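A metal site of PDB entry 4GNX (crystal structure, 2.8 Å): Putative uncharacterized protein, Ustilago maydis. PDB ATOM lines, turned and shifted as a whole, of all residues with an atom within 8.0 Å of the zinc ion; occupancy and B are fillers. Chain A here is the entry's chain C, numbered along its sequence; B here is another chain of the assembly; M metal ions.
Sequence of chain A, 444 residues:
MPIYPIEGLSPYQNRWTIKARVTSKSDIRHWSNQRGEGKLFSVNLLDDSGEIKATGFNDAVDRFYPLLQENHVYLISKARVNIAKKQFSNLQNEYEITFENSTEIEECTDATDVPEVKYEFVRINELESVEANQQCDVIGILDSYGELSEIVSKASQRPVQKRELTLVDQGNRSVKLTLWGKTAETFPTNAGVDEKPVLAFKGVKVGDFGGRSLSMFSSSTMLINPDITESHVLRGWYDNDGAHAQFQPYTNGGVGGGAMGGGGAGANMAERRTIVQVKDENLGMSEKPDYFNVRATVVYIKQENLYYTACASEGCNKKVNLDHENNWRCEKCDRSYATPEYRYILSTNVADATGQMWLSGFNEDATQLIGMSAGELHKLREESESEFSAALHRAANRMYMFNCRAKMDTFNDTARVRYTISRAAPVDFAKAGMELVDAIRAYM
The nearest printed residue that does not touch the zinc ion is Ser 313 (4.1 Å).
The zinc ion is bound by the side-chain sulfur of Cys 311 (2.3 Å), the side-chain sulfur of Cys 333 (2.3 Å), the side-chain sulfur of Cys 330 (2.3 Å) and the side-chain sulfur of Cys 316 (2.3 Å).
The zinc ion has four donor atoms within binding distance.
The side-chain sulfur of Cys 311 sits close to the backbone NH of Ser 313 (3.3 Å).
The backbone carbonyl oxygen of Lys 318 is in hydrogen-bond range of the backbone NH of Cys 311 (3.1 Å).
SG of Cys 333 lies close to OG of Ser 313, at 3.1 Å.
The backbone NH (N) of Lys 332 sits close to the side-chain sulfur (SG) of Cys 330, 3.7 Å away.
The backbone carbonyl oxygen of Arg 335 lies within hydrogen-bond range of the backbone NH of Cys 330 (3.0 Å).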
ATOM      1  N   ALA A 310     -22.138   2.939  24.063  1.00  0.00           N
ATOM      2  CA  ALA A 310     -23.224   2.059  23.606  1.00  0.00           C
ATOM      3  C   ALA A 310     -22.949   1.271  22.318  1.00  0.00           C
ATOM      4  O   ALA A 310     -22.047   1.611  21.542  1.00  0.00           O
ATOM      5  CB  ALA A 310     -24.527   2.848  23.488  1.00  0.00           C
ATOM      6  N   CYS A 311     -23.752   0.235  22.081  1.00  0.00           N
ATOM      7  CA  CYS A 311     -23.549  -0.715  20.990  1.00  0.00           C
ATOM      8  C   CYS A 311     -23.803  -0.107  19.623  1.00  0.00           C
ATOM      9  O   CYS A 311     -24.809   0.575  19.431  1.00  0.00           O
ATOM     10  CB  CYS A 311     -24.475  -1.916  21.185  1.00  0.00           C
ATOM     11  SG  CYS A 311     -24.543  -3.151  19.851  1.00  0.00           S
ATOM     12  N   ALA A 312     -22.892  -0.370  18.698  1.00  0.00           N
ATOM     13  CA  ALA A 312     -22.984   0.172  17.336  1.00  0.00           C
ATOM     14  C   ALA A 312     -23.949  -0.591  16.403  1.00  0.00           C
ATOM     15  O   ALA A 312     -23.948  -0.370  15.179  1.00  0.00           O
ATOM     16  CB  ALA A 312     -21.594   0.302  16.718  1.00  0.00           C
ATOM     17  N   SER A 313     -24.775  -1.462  16.980  1.00  0.00           N
ATOM     18  CA  SER A 313     -25.769  -2.187  16.200  1.00  0.00           C
ATOM     19  C   SER A 313     -26.956  -1.303  15.921  1.00  0.00           C
ATOM     20  O   SER A 313     -27.391  -0.547  16.793  1.00  0.00           O
ATOM     21  CB  SER A 313     -26.263  -3.453  16.923  1.00  0.00           C
ATOM     22  OG  SER A 313     -25.428  -4.571  16.667  1.00  0.00           O
ATOM     23  N   GLU A 314     -27.464  -1.394  14.688  1.00  0.00           N
ATOM     24  CA  GLU A 314     -28.729  -0.780  14.308  1.00  0.00           C
ATOM     25  C   GLU A 314     -29.821  -1.216  15.284  1.00  0.00           C
ATOM     26  O   GLU A 314     -29.988  -2.421  15.547  1.00  0.00           O
ATOM     27  CB  GLU A 314     -29.082  -1.153  12.852  1.00  0.00           C
ATOM     28  CG  GLU A 314     -30.501  -0.805  12.402  1.00  0.00           C
ATOM     29  CD  GLU A 314     -30.823   0.682  12.494  1.00  0.00           C
ATOM     30  OE1 GLU A 314     -29.884   1.507  12.568  1.00  0.00           O
ATOM     31  OE2 GLU A 314     -32.034   1.018  12.491  1.00  0.00           O
ATOM     32  N   GLY A 315     -30.532  -0.249  15.842  1.00  0.00           N
ATOM     33  CA  GLY A 315     -31.645  -0.531  16.743  1.00  0.00           C
ATOM     34  C   GLY A 315     -31.258  -0.818  18.177  1.00  0.00           C
ATOM     35  O   GLY A 315     -32.080  -0.650  19.086  1.00  0.00           O
ATOM     36  N   CYS A 316     -30.003  -1.246  18.388  1.00  0.00           N
ATOM     37  CA  CYS A 316     -29.495  -1.651  19.717  1.00  0.00           C
ATOM     38  C   CYS A 316     -28.748  -0.526  20.471  1.00  0.00           C
ATOM     39  O   CYS A 316     -27.952   0.225  19.888  1.00  0.00           O
ATOM     40  CB  CYS A 316     -28.607  -2.902  19.591  1.00  0.00           C
ATOM     41  SG  CYS A 316     -28.049  -3.635  21.161  1.00  0.00           S
ATOM     42  N   ASN A 317     -29.032  -0.434  21.783  1.00  0.00           N
ATOM     43  CA  ASN A 317     -28.501   0.638  22.639  1.00  0.00           C
ATOM     44  C   ASN A 317     -27.821   0.167  23.923  1.00  0.00           C
ATOM     45  O   ASN A 317     -27.335   0.996  24.701  1.00  0.00           O
ATOM     46  CB  ASN A 317     -29.611   1.614  23.060  1.00  0.00           C
ATOM     47  CG  ASN A 317     -30.359   2.214  21.890  1.00  0.00           C
ATOM     48  OD1 ASN A 317     -29.847   2.279  20.758  1.00  0.00           O
ATOM     49  ND2 ASN A 317     -31.577   2.671  22.149  1.00  0.00           N
ATOM     50  N   LYS A 318     -27.800  -1.149  24.174  1.00  0.00           N
ATOM     51  CA  LYS A 318     -27.206  -1.698  25.398  1.00  0.00           C
ATOM     52  C   LYS A 318     -25.772  -1.165  25.592  1.00  0.00           C
ATOM     53  O   LYS A 318     -25.104  -0.804  24.634  1.00  0.00           O
ATOM     54  CB  LYS A 318     -27.259  -3.241  25.360  1.00  0.00           C
ATOM     55  CG  LYS A 318     -26.412  -3.973  26.402  1.00  0.00           C
ATOM     56  CD  LYS A 318     -26.850  -3.724  27.849  1.00  0.00           C
ATOM     57  CE  LYS A 318     -25.661  -3.700  28.818  1.00  0.00           C
ATOM     58  NZ  LYS A 318     -26.021  -3.965  30.245  1.00  0.00           N
ATOM     59  N   LYS A 319     -25.326  -1.064  26.839  1.00  0.00           N
ATOM     60  CA  LYS A 319     -23.951  -0.656  27.150  1.00  0.00           C
ATOM     61  C   LYS A 319     -22.933  -1.711  26.717  1.00  0.00           C
ATOM     62  O   LYS A 319     -23.137  -2.915  26.925  1.00  0.00           O
ATOM     63  CB  LYS A 319     -23.787  -0.376  28.657  1.00  0.00           C
ATOM     64  CG  LYS A 319     -22.448   0.263  29.011  1.00  0.00           C
ATOM     65  CD  LYS A 319     -22.222   0.369  30.501  1.00  0.00           C
ATOM     66  CE  LYS A 319     -20.810   0.852  30.773  1.00  0.00           C
ATOM     67  NZ  LYS A 319     -20.698   1.412  32.144  1.00  0.00           N
ATOM     68  N   VAL A 320     -21.839  -1.250  26.119  1.00  0.00           N
ATOM     69  CA  VAL A 320     -20.705  -2.102  25.721  1.00  0.00           C
ATOM     70  C   VAL A 320     -19.490  -1.931  26.663  1.00  0.00           C
ATOM     71  O   VAL A 320     -19.409  -0.946  27.391  1.00  0.00           O
ATOM     72  CB  VAL A 320     -20.288  -1.876  24.245  1.00  0.00           C
ATOM     73  CG1 VAL A 320     -21.403  -2.281  23.302  1.00  0.00           C
ATOM     74  CG2 VAL A 320     -19.862  -0.424  23.994  1.00  0.00           C
ATOM     75  N   ARG A 329     -17.109  -4.653  23.276  1.00  0.00           N
ATOM     76  CA  ARG A 329     -18.029  -5.794  23.151  1.00  0.00           C
ATOM     77  C   ARG A 329     -19.474  -5.554  23.650  1.00  0.00           C
ATOM     78  O   ARG A 329     -19.670  -5.091  24.792  1.00  0.00           O
ATOM     79  CB  ARG A 329     -17.439  -7.072  23.775  1.00  0.00           C
ATOM     80  CG  ARG A 329     -18.393  -8.260  23.722  1.00  0.00           C
ATOM     81  CD  ARG A 329     -17.709  -9.615  23.739  1.00  0.00           C
ATOM     82  NE  ARG A 329     -18.588 -10.655  23.184  1.00  0.00           N
ATOM     83  CZ  ARG A 329     -19.448 -11.399  23.886  1.00  0.00           C
ATOM     84  NH1 ARG A 329     -19.565 -11.250  25.197  1.00  0.00           N
ATOM     85  NH2 ARG A 329     -20.201 -12.303  23.274  1.00  0.00           N
ATOM     86  N   CYS A 330     -20.460  -5.894  22.804  1.00  0.00           N
ATOM     87  CA  CYS A 330     -21.873  -5.992  23.203  1.00  0.00           C
ATOM     88  C   CYS A 330     -22.222  -7.430  23.558  1.00  0.00           C
ATOM     89  O   CYS A 330     -21.807  -8.360  22.869  1.00  0.00           O
ATOM     90  CB  CYS A 330     -22.808  -5.513  22.073  1.00  0.00           C
ATOM     91  SG  CYS A 330     -24.561  -5.539  22.522  1.00  0.00           S
ATOM     92  N   GLU A 331     -23.007  -7.604  24.616  1.00  0.00           N
ATOM     93  CA  GLU A 331     -23.480  -8.939  25.014  1.00  0.00           C
ATOM     94  C   GLU A 331     -24.610  -9.420  24.114  1.00  0.00           C
ATOM     95  O   GLU A 331     -24.475 -10.437  23.420  1.00  0.00           O
ATOM     96  CB  GLU A 331     -23.925  -8.979  26.489  1.00  0.00           C
ATOM     97  CG  GLU A 331     -22.825  -8.840  27.528  1.00  0.00           C
ATOM     98  CD  GLU A 331     -21.597  -9.667  27.187  1.00  0.00           C
ATOM     99  OE1 GLU A 331     -20.772  -9.206  26.376  1.00  0.00           O
ATOM    100  OE2 GLU A 331     -21.451 -10.764  27.751  1.00  0.00           O
ATOM    101  N   LYS A 332     -25.721  -8.675  24.125  1.00  0.00           N
ATOM    102  CA  LYS A 332     -26.943  -8.999  23.394  1.00  0.00           C
ATOM    103  C   LYS A 332     -26.658  -9.371  21.949  1.00  0.00           C
ATOM    104  O   LYS A 332     -27.074 -10.454  21.472  1.00  0.00           O
ATOM    105  CB  LYS A 332     -27.930  -7.816  23.412  1.00  0.00           C
ATOM    106  CG  LYS A 332     -29.258  -8.075  22.689  1.00  0.00           C
ATOM    107  CD  LYS A 332     -29.542  -7.015  21.631  1.00  0.00           C
ATOM    108  CE  LYS A 332     -31.004  -6.959  21.232  1.00  0.00           C
ATOM    109  NZ  LYS A 332     -31.859  -6.311  22.267  1.00  0.00           N
ATOM    110  N   CYS A 333     -25.965  -8.484  21.244  1.00  0.00           N
ATOM    111  CA  CYS A 333     -25.671  -8.743  19.843  1.00  0.00           C
ATOM    112  C   CYS A 333     -24.333  -9.467  19.633  1.00  0.00           C
ATOM    113  O   CYS A 333     -23.940  -9.752  18.497  1.00  0.00           O
ATOM    114  CB  CYS A 333     -25.895  -7.508  18.943  1.00  0.00           C
ATOM    115  SG  CYS A 333     -24.904  -6.056  19.291  1.00  0.00           S
ATOM    116  N   ASP A 334     -23.667  -9.802  20.740  1.00  0.00           N
ATOM    117  CA  ASP A 334     -22.549 -10.756  20.751  1.00  0.00           C
ATOM    118  C   ASP A 334     -21.558 -10.444  19.621  1.00  0.00           C
ATOM    119  O   ASP A 334     -21.484 -11.159  18.620  1.00  0.00           O
ATOM    120  CB  ASP A 334     -23.102 -12.194  20.663  1.00  0.00           C
ATOM    121  CG  ASP A 334     -22.018 -13.262  20.775  1.00  0.00           C
ATOM    122  OD1 ASP A 334     -20.816 -12.935  20.895  1.00  0.00           O
ATOM    123  OD2 ASP A 334     -22.376 -14.462  20.731  1.00  0.00           O
ATOM    124  N   ARG A 335     -20.790  -9.370  19.795  1.00  0.00           N
ATOM    125  CA  ARG A 335     -19.869  -8.866  18.785  1.00  0.00           C
ATOM    126  C   ARG A 335     -19.054  -7.698  19.361  1.00  0.00           C
ATOM    127  O   ARG A 335     -19.234  -7.331  20.525  1.00  0.00           O
ATOM    128  CB  ARG A 335     -20.628  -8.411  17.546  1.00  0.00           C
ATOM    129  CG  ARG A 335     -19.768  -8.280  16.305  1.00  0.00           C
ATOM    130  CD  ARG A 335     -20.385  -7.344  15.290  1.00  0.00           C
ATOM    131  NE  ARG A 335     -19.536  -7.347  14.099  1.00  0.00           N
ATOM    132  CZ  ARG A 335     -18.724  -6.369  13.745  1.00  0.00           C
ATOM    133  NH1 ARG A 335     -18.660  -5.260  14.464  1.00  0.00           N
ATOM    134  NH2 ARG A 335     -17.982  -6.493  12.655  1.00  0.00           N
ATOM    135  N   TYR A 337     -16.845  -3.799  18.225  1.00  0.00           N
ATOM    136  CA  TYR A 337     -16.546  -2.706  17.315  1.00  0.00           C
ATOM    137  C   TYR A 337     -15.347  -1.910  17.856  1.00  0.00           C
ATOM    138  O   TYR A 337     -15.177  -1.785  19.076  1.00  0.00           O
ATOM    139  CB  TYR A 337     -17.754  -1.786  17.218  1.00  0.00           C
ATOM    140  CG  TYR A 337     -19.052  -2.463  16.833  1.00  0.00           C
ATOM    141  CD1 TYR A 337     -19.845  -3.097  17.787  1.00  0.00           C
ATOM    142  CD2 TYR A 337     -19.492  -2.432  15.514  1.00  0.00           C
ATOM    143  CE1 TYR A 337     -21.043  -3.711  17.427  1.00  0.00           C
ATOM    144  CE2 TYR A 337     -20.688  -3.027  15.138  1.00  0.00           C
ATOM    145  CZ  TYR A 337     -21.458  -3.670  16.092  1.00  0.00           C
ATOM    146  OH  TYR A 337     -22.631  -4.262  15.687  1.00  0.00           O
ATOM    147  P    DT B  13     -31.645  -1.303  25.187  1.00  0.00           P
ATOM    148  OP1  DT B  13     -30.336  -1.118  24.507  1.00  0.00           O
ATOM    149  OP2  DT B  13     -32.174  -2.686  25.344  1.00  0.00           O
ATOM    150  O5'  DT B  13     -31.589  -0.599  26.618  1.00  0.00           O
ATOM    151  C5'  DT B  13     -30.385  -0.524  27.408  1.00  0.00           C
ATOM    152  C4'  DT B  13     -29.895   0.906  27.526  1.00  0.00           C
ATOM    153  O4'  DT B  13     -30.778   1.791  26.816  1.00  0.00           O
ATOM    154  C3'  DT B  13     -29.845   1.462  28.941  1.00  0.00           C
ATOM    155  O3'  DT B  13     -28.526   1.322  29.449  1.00  0.00           O
ATOM    156  C2'  DT B  13     -30.067   2.957  28.748  1.00  0.00           C
ATOM    157  C1'  DT B  13     -30.658   3.101  27.349  1.00  0.00           C
ATOM    158  N1   DT B  13     -31.991   3.717  27.339  1.00  0.00           N
ATOM    159  C2   DT B  13     -32.289   4.647  26.367  1.00  0.00           C
ATOM    160  O2   DT B  13     -31.484   5.012  25.522  1.00  0.00           O
ATOM    161  N3   DT B  13     -33.566   5.144  26.435  1.00  0.00           N
ATOM    162  C4   DT B  13     -34.558   4.801  27.345  1.00  0.00           C
ATOM    163  O4   DT B  13     -35.656   5.337  27.285  1.00  0.00           O
ATOM    164  C5   DT B  13     -34.168   3.812  28.338  1.00  0.00           C
ATOM    165  C7   DT B  13     -35.164   3.384  29.362  1.00  0.00           C
ATOM    166  C6   DT B  13     -32.923   3.323  28.274  1.00  0.00           C
HETATM  167 ZN    ZN M   1     -25.965  -4.674  20.855  1.00  0.00          ZN
